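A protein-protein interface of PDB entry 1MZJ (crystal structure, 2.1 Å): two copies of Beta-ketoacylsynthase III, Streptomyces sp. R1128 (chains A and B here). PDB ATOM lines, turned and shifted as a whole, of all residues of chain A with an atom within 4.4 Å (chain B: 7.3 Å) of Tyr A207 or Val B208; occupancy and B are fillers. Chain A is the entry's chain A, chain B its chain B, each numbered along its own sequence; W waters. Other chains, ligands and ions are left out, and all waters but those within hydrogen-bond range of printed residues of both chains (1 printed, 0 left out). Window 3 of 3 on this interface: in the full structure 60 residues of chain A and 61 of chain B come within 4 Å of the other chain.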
ATOM      1  N   SER A 203      10.079  18.056   6.229  1.00  0.00           N
ATOM      2  CA  SER A 203       8.854  17.442   6.726  1.00  0.00           C
ATOM      3  C   SER A 203       7.777  18.551   6.868  1.00  0.00           C
ATOM      4  O   SER A 203       8.092  19.751   6.862  1.00  0.00           O
ATOM      5  CB  SER A 203       9.066  16.823   8.091  1.00  0.00           C
ATOM      6  OG  SER A 203       9.377  17.845   8.992  1.00  0.00           O
ATOM      7  N   TRP A 204       6.507  18.172   6.988  1.00  0.00           N
ATOM      8  CA  TRP A 204       5.520  19.221   7.066  1.00  0.00           C
ATOM      9  C   TRP A 204       5.728  20.099   8.304  1.00  0.00           C
ATOM     10  O   TRP A 204       5.295  21.255   8.324  1.00  0.00           O
ATOM     11  CB  TRP A 204       4.097  18.648   7.044  1.00  0.00           C
ATOM     12  CG  TRP A 204       3.724  18.149   5.691  1.00  0.00           C
ATOM     13  CD1 TRP A 204       3.620  16.835   5.293  1.00  0.00           C
ATOM     14  CD2 TRP A 204       3.509  18.947   4.521  1.00  0.00           C
ATOM     15  NE1 TRP A 204       3.360  16.778   3.942  1.00  0.00           N
ATOM     16  CE2 TRP A 204       3.290  18.055   3.441  1.00  0.00           C
ATOM     17  CE3 TRP A 204       3.481  20.325   4.279  1.00  0.00           C
ATOM     18  CZ2 TRP A 204       3.055  18.501   2.141  1.00  0.00           C
ATOM     19  CZ3 TRP A 204       3.247  20.771   2.990  1.00  0.00           C
ATOM     20  CH2 TRP A 204       3.038  19.859   1.929  1.00  0.00           C
ATOM     21  N   ASP A 205       6.383  19.489   9.302  1.00  0.00           N
ATOM     22  CA  ASP A 205       6.730  20.061  10.601  1.00  0.00           C
ATOM     23  C   ASP A 205       7.618  21.238  10.338  1.00  0.00           C
ATOM     24  O   ASP A 205       7.348  22.331  10.810  1.00  0.00           O
ATOM     25  CB  ASP A 205       7.500  19.026  11.431  1.00  0.00           C
ATOM     26  CG  ASP A 205       6.730  18.558  12.641  1.00  0.00           C
ATOM     27  OD1 ASP A 205       7.218  17.621  13.342  1.00  0.00           O
ATOM     28  OD2 ASP A 205       5.640  19.135  12.890  1.00  0.00           O
ATOM     29  N   GLN A 206       8.683  21.009   9.584  1.00  0.00           N
ATOM     30  CA  GLN A 206       9.603  22.067   9.228  1.00  0.00           C
ATOM     31  C   GLN A 206       8.988  23.065   8.252  1.00  0.00           C
ATOM     32  O   GLN A 206       9.474  24.180   8.126  1.00  0.00           O
ATOM     33  CB  GLN A 206      10.871  21.503   8.603  1.00  0.00           C
ATOM     34  CG  GLN A 206      11.623  20.564   9.487  1.00  0.00           C
ATOM     35  CD  GLN A 206      12.637  19.806   8.694  1.00  0.00           C
ATOM     36  OE1 GLN A 206      12.316  19.231   7.661  1.00  0.00           O
ATOM     37  NE2 GLN A 206      13.875  19.808   9.158  1.00  0.00           N
ATOM     38  N   TYR A 207       7.951  22.660   7.539  1.00  0.00           N
ATOM     39  CA  TYR A 207       7.302  23.562   6.607  1.00  0.00           C
ATOM     40  C   TYR A 207       6.532  24.572   7.450  1.00  0.00           C
ATOM     41  O   TYR A 207       6.626  25.770   7.226  1.00  0.00           O
ATOM     42  CB  TYR A 207       6.324  22.815   5.702  1.00  0.00           C
ATOM     43  CG  TYR A 207       5.602  23.728   4.757  1.00  0.00           C
ATOM     44  CD1 TYR A 207       4.257  24.011   4.923  1.00  0.00           C
ATOM     45  CD2 TYR A 207       6.294  24.361   3.723  1.00  0.00           C
ATOM     46  CE1 TYR A 207       3.608  24.913   4.079  1.00  0.00           C
ATOM     47  CE2 TYR A 207       5.660  25.260   2.873  1.00  0.00           C
ATOM     48  CZ  TYR A 207       4.318  25.532   3.051  1.00  0.00           C
ATOM     49  OH  TYR A 207       3.681  26.385   2.171  1.00  0.00           O
ATOM     50  N   VAL A 208       5.773  24.075   8.419  1.00  0.00           N
ATOM     51  CA  VAL A 208       4.843  24.822   9.285  1.00  0.00           C
ATOM     52  C   VAL A 208       5.574  25.889  10.119  1.00  0.00           C
ATOM     53  O   VAL A 208       4.971  26.794  10.697  1.00  0.00           O
ATOM     54  CB  VAL A 208       4.065  23.840  10.218  1.00  0.00           C
ATOM     55  CG1 VAL A 208       3.519  24.494  11.512  1.00  0.00           C
ATOM     56  CG2 VAL A 208       2.895  23.248   9.481  1.00  0.00           C
ATOM     57  N   GLU A 209       6.908  25.778  10.127  1.00  0.00           N
ATOM     58  CA  GLU A 209       7.714  26.565  11.080  1.00  0.00           C
ATOM     59  C   GLU A 209       8.465  27.735  10.423  1.00  0.00           C
ATOM     60  O   GLU A 209       8.947  28.632  11.111  1.00  0.00           O
ATOM     61  CB  GLU A 209       8.721  25.618  11.781  1.00  0.00           C
ATOM     62  CG  GLU A 209       8.251  25.208  13.180  1.00  0.00           C
ATOM     63  CD  GLU A 209       8.654  26.250  14.196  1.00  0.00           C
ATOM     64  OE1 GLU A 209       9.840  26.510  14.325  1.00  0.00           O
ATOM     65  OE2 GLU A 209       7.768  26.756  14.884  1.00  0.00           O
ATOM     66  N   ASP A 210       8.565  27.675   9.065  1.00  0.00           N
ATOM     67  CA  ASP A 210       9.430  28.606   8.293  1.00  0.00           C
ATOM     68  C   ASP A 210       9.183  28.390   6.788  1.00  0.00           C
ATOM     69  O   ASP A 210       9.386  27.308   6.264  1.00  0.00           O
ATOM     70  CB  ASP A 210      10.905  28.282   8.676  1.00  0.00           C
ATOM     71  CG  ASP A 210      12.007  29.238   8.139  1.00  0.00           C
ATOM     72  OD1 ASP A 210      11.797  30.454   8.076  1.00  0.00           O
ATOM     73  OD2 ASP A 210      13.112  28.755   7.916  1.00  0.00           O
ATOM     74  N   PRO A 211       8.571  29.410   6.084  1.00  0.00           N
ATOM     75  CA  PRO A 211       8.781  29.611   4.644  1.00  0.00           C
ATOM     76  C   PRO A 211       9.818  30.708   4.370  1.00  0.00           C
ATOM     77  O   PRO A 211       9.836  31.747   5.040  1.00  0.00           O
ATOM     78  CB  PRO A 211       7.426  30.015   4.059  1.00  0.00           C
ATOM     79  CG  PRO A 211       6.524  30.460   5.222  1.00  0.00           C
ATOM     80  CD  PRO A 211       7.516  30.303   6.488  1.00  0.00           C
ATOM     81  N   VAL A 213      11.496  26.965   2.476  1.00  0.00           N
ATOM     82  CA  VAL A 213      11.655  25.629   3.039  1.00  0.00           C
ATOM     83  C   VAL A 213      10.927  24.794   1.991  1.00  0.00           C
ATOM     84  O   VAL A 213      11.206  23.636   1.727  1.00  0.00           O
ATOM     85  CB  VAL A 213      10.867  25.566   4.352  1.00  0.00           C
ATOM     86  CG1 VAL A 213       9.352  25.452   4.055  1.00  0.00           C
ATOM     87  CG2 VAL A 213      11.321  24.397   5.180  1.00  0.00           C
ATOM     88  N   GLY A 214       9.912  25.481   1.422  1.00  0.00           N
ATOM     89  CA  GLY A 214       8.958  24.905   0.493  1.00  0.00           C
ATOM     90  C   GLY A 214       8.182  23.753   1.087  1.00  0.00           C
ATOM     91  O   GLY A 214       8.496  23.244   2.149  1.00  0.00           O
ATOM     92  N   ARG A 215       7.124  23.359   0.368  1.00  0.00           N
ATOM     93  CA  ARG A 215       6.477  22.065   0.552  1.00  0.00           C
ATOM     94  C   ARG A 215       7.454  20.910   0.319  1.00  0.00           C
ATOM     95  O   ARG A 215       8.261  20.913  -0.602  1.00  0.00           O
ATOM     96  CB  ARG A 215       5.317  21.968  -0.439  1.00  0.00           C
ATOM     97  CG  ARG A 215       5.787  22.067  -1.891  1.00  0.00           C
ATOM     98  CD  ARG A 215       4.748  21.515  -2.874  1.00  0.00           C
ATOM     99  NE  ARG A 215       3.485  22.250  -2.755  1.00  0.00           N
ATOM    100  CZ  ARG A 215       2.486  21.648  -2.084  1.00  0.00           C
ATOM    101  NH1 ARG A 215       2.667  20.449  -1.559  1.00  0.00           N
ATOM    102  NH2 ARG A 215       1.309  22.268  -1.952  1.00  0.00           N
ATOM    103  N   SER B 203      -5.855  19.092   4.730  1.00  0.00           N
ATOM    104  CA  SER B 203      -4.792  18.261   4.209  1.00  0.00           C
ATOM    105  C   SER B 203      -3.614  19.215   4.010  1.00  0.00           C
ATOM    106  O   SER B 203      -3.802  20.431   3.771  1.00  0.00           O
ATOM    107  CB  SER B 203      -5.206  17.660   2.870  1.00  0.00           C
ATOM    108  OG  SER B 203      -5.336  18.690   1.913  1.00  0.00           O
ATOM    109  N   TRP B 204      -2.399  18.693   4.092  1.00  0.00           N
ATOM    110  CA  TRP B 204      -1.254  19.575   3.926  1.00  0.00           C
ATOM    111  C   TRP B 204      -1.283  20.315   2.607  1.00  0.00           C
ATOM    112  O   TRP B 204      -0.677  21.370   2.474  1.00  0.00           O
ATOM    113  CB  TRP B 204       0.062  18.799   4.064  1.00  0.00           C
ATOM    114  CG  TRP B 204       0.282  18.367   5.444  1.00  0.00           C
ATOM    115  CD1 TRP B 204       0.062  17.123   5.967  1.00  0.00           C
ATOM    116  CD2 TRP B 204       0.664  19.196   6.528  1.00  0.00           C
ATOM    117  NE1 TRP B 204       0.287  17.134   7.316  1.00  0.00           N
ATOM    118  CE2 TRP B 204       0.658  18.394   7.688  1.00  0.00           C
ATOM    119  CE3 TRP B 204       1.009  20.548   6.634  1.00  0.00           C
ATOM    120  CZ2 TRP B 204       0.987  18.888   8.934  1.00  0.00           C
ATOM    121  CZ3 TRP B 204       1.337  21.040   7.869  1.00  0.00           C
ATOM    122  CH2 TRP B 204       1.325  20.207   9.013  1.00  0.00           C
ATOM    123  N   ASP B 205      -2.016  19.754   1.652  1.00  0.00           N
ATOM    124  CA  ASP B 205      -2.132  20.294   0.304  1.00  0.00           C
ATOM    125  C   ASP B 205      -2.890  21.594   0.361  1.00  0.00           C
ATOM    126  O   ASP B 205      -2.603  22.526  -0.383  1.00  0.00           O
ATOM    127  CB  ASP B 205      -2.886  19.302  -0.591  1.00  0.00           C
ATOM    128  CG  ASP B 205      -2.285  19.190  -1.957  1.00  0.00           C
ATOM    129  OD1 ASP B 205      -2.829  18.408  -2.781  1.00  0.00           O
ATOM    130  OD2 ASP B 205      -1.264  19.879  -2.207  1.00  0.00           O
ATOM    131  N   GLN B 206      -3.859  21.648   1.266  1.00  0.00           N
ATOM    132  CA  GLN B 206      -4.676  22.844   1.431  1.00  0.00           C
ATOM    133  C   GLN B 206      -3.897  23.880   2.199  1.00  0.00           C
ATOM    134  O   GLN B 206      -3.905  25.067   1.853  1.00  0.00           O
ATOM    135  CB  GLN B 206      -5.966  22.502   2.160  1.00  0.00           C
ATOM    136  CG  GLN B 206      -6.753  21.435   1.426  1.00  0.00           C
ATOM    137  CD  GLN B 206      -7.951  20.981   2.188  1.00  0.00           C
ATOM    138  OE1 GLN B 206      -7.876  20.730   3.391  1.00  0.00           O
ATOM    139  NE2 GLN B 206      -9.079  20.854   1.495  1.00  0.00           N
ATOM    140  N   TYR B 207      -3.201  23.408   3.225  1.00  0.00           N
ATOM    141  CA  TYR B 207      -2.392  24.265   4.053  1.00  0.00           C
ATOM    142  C   TYR B 207      -1.507  25.079   3.114  1.00  0.00           C
ATOM    143  O   TYR B 207      -1.138  26.208   3.434  1.00  0.00           O
ATOM    144  CB  TYR B 207      -1.572  23.412   5.033  1.00  0.00           C
ATOM    145  CG  TYR B 207      -0.753  24.213   6.005  1.00  0.00           C
ATOM    146  CD1 TYR B 207       0.601  24.445   5.796  1.00  0.00           C
ATOM    147  CD2 TYR B 207      -1.347  24.778   7.119  1.00  0.00           C
ATOM    148  CE1 TYR B 207       1.330  25.222   6.669  1.00  0.00           C
ATOM    149  CE2 TYR B 207      -0.629  25.551   7.996  1.00  0.00           C
ATOM    150  CZ  TYR B 207       0.697  25.774   7.769  1.00  0.00           C
ATOM    151  OH  TYR B 207       1.385  26.564   8.639  1.00  0.00           O
ATOM    152  N   VAL B 208      -1.155  24.515   1.961  1.00  0.00           N
ATOM    153  CA  VAL B 208      -0.367  25.250   0.969  1.00  0.00           C
ATOM    154  C   VAL B 208      -1.257  25.644  -0.199  1.00  0.00           C
ATOM    155  O   VAL B 208      -1.296  24.955  -1.221  1.00  0.00           O
ATOM    156  CB  VAL B 208       0.760  24.409   0.362  1.00  0.00           C
ATOM    157  CG1 VAL B 208       1.546  25.235  -0.629  1.00  0.00           C
ATOM    158  CG2 VAL B 208       1.651  23.899   1.441  1.00  0.00           C
ATOM    159  N   GLU B 209      -1.941  26.763  -0.078  1.00  0.00           N
ATOM    160  CA  GLU B 209      -2.872  27.201  -1.105  1.00  0.00           C
ATOM    161  C   GLU B 209      -3.749  28.159  -0.352  1.00  0.00           C
ATOM    162  O   GLU B 209      -4.021  29.248  -0.835  1.00  0.00           O
ATOM    163  CB  GLU B 209      -3.757  26.034  -1.580  1.00  0.00           C
ATOM    164  CG  GLU B 209      -4.067  26.020  -3.067  1.00  0.00           C
ATOM    165  CD  GLU B 209      -5.470  26.504  -3.365  1.00  0.00           C
ATOM    166  OE1 GLU B 209      -6.032  27.289  -2.567  1.00  0.00           O
ATOM    167  OE2 GLU B 209      -6.020  26.100  -4.407  1.00  0.00           O
ATOM    168  N   ASP B 210      -4.363  27.764   0.704  1.00  0.00           N
ATOM    169  CA  ASP B 210      -4.953  28.656   1.697  1.00  0.00           C
ATOM    170  C   ASP B 210      -4.549  28.373   3.124  1.00  0.00           C
ATOM    171  O   ASP B 210      -5.058  27.439   3.733  1.00  0.00           O
ATOM    172  CB  ASP B 210      -6.478  28.529   1.620  1.00  0.00           C
ATOM    173  CG  ASP B 210      -7.176  29.263   2.781  1.00  0.00           C
ATOM    174  OD1 ASP B 210      -7.360  30.503   2.713  1.00  0.00           O
ATOM    175  OD2 ASP B 210      -7.514  28.589   3.779  1.00  0.00           O
ATOM    176  N   PRO B 211      -3.626  29.170   3.674  1.00  0.00           N
ATOM    177  CA  PRO B 211      -3.170  28.985   5.055  1.00  0.00           C
ATOM    178  C   PRO B 211      -4.315  29.112   6.048  1.00  0.00           C
ATOM    179  O   PRO B 211      -4.323  28.436   7.078  1.00  0.00           O
ATOM    180  CB  PRO B 211      -2.095  30.056   5.239  1.00  0.00           C
ATOM    181  CG  PRO B 211      -2.149  30.900   3.979  1.00  0.00           C
ATOM    182  CD  PRO B 211      -2.726  30.048   2.919  1.00  0.00           C
ATOM    183  N   VAL B 213      -7.036  27.778   6.652  1.00  0.00           N
ATOM    184  CA  VAL B 213      -7.349  26.495   7.314  1.00  0.00           C
ATOM    185  C   VAL B 213      -6.003  25.809   7.361  1.00  0.00           C
ATOM    186  O   VAL B 213      -5.609  25.095   6.427  1.00  0.00           O
ATOM    187  CB  VAL B 213      -8.302  25.600   6.502  1.00  0.00           C
ATOM    188  CG1 VAL B 213      -9.671  25.556   7.178  1.00  0.00           C
ATOM    189  CG2 VAL B 213      -8.395  26.099   5.065  1.00  0.00           C
ATOM    190  N   GLY B 214      -5.294  26.037   8.459  1.00  0.00           N
ATOM    191  CA  GLY B 214      -3.871  25.711   8.456  1.00  0.00           C
ATOM    192  C   GLY B 214      -3.584  24.375   9.151  1.00  0.00           C
ATOM    193  O   GLY B 214      -4.475  23.630   9.534  1.00  0.00           O
HETATM  194  O   HOH W   1      -1.283  22.899  -2.774  1.00  0.00           O
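Trp A204 touches its own counterpart, Trp B204.
Trp A204 touches Val B208, and with the chains exchanged Val A208 touches Trp B204.
Tyr A207 touches its own counterpart, Tyr B207.
Tyr A207 touches Val B208, and with the chains exchanged Val A208 touches Tyr B207.
Of the 8 pairs that touch across the chains among the printed residues, 6 have their exchanged pair printed and touching as well.
Of chain B, only Tyr B207 and Val B208 come within 4 Å of Tyr A207.
Of chain A, only Trp A204 (3.8 Å), Tyr A207 (3.3 Å) and Arg A215 (3.2 Å) come within 4 Å of Val B208.
Of the printed residues of chain A, Trp B204 touches Trp A204 (3.3 Å) and Val A208 (3.1 Å).
Printed residues of chain A within 4 Å of Asp B205: Arg A215.
Of the printed residues of chain B, Val A208 touches Trp B204 (3.1 Å) and Tyr B207 (3.7 Å).
Ser A203 touches none of the printed residues of chain B.
Asp A210 touches none of the printed residues of chain B.
The nearest residue of chain B that does not touch Tyr A207 is Trp B204 (5.0 Å).
The side-chain hydroxyl of Ser B203 sits close to the backbone NH of Asp B205 (3.5 Å).
Among the printed residues, merely in contact across the chains: Val A208 with Trp B204, Arg A215 with Val B208, Tyr A207 with Val B208, Trp A204 with Trp B204, Tyr A207 with Tyr B207, Val A208 with Tyr B207 and Trp A204 with Val B208.
Of the 11 printed residues of chain B, 4 touch a printed residue of chain A.
Hydrophobic or aromatic side chains of chain B within 4 Å of the printed part of chain A: Trp B204, Tyr B207 and Val B208.
Of the 12 printed residues of chain A, 4 touch a printed residue of chain B.
Printed residues of chain A that touch a printed residue of chain B: Trp A204, Tyr A207, Val A208 and Arg A215.
Hydrophobic or aromatic side chains of chain A that line the printed part of chain B: Trp A204, Tyr A207 and Val A208.
Among the printed residues, Asp or Glu carboxylates within 4 Å of a Lys or Arg side-chain nitrogen of the other chain: Arg A215 with Asp B205 (3.5 Å).
Water W1 lies within hydrogen-bond range of the backbone carbonyl oxygen (O) of Val B208 (2.6 Å), the backbone carbonyl oxygen (O) of Asp B205 (2.8 Å) and the guanidinium group (NH2) of Arg A215 (2.8 Å).
OD2 of Asp B205 lies within salt-bridge range of NH2 of Arg A215, at 3.5 Å.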
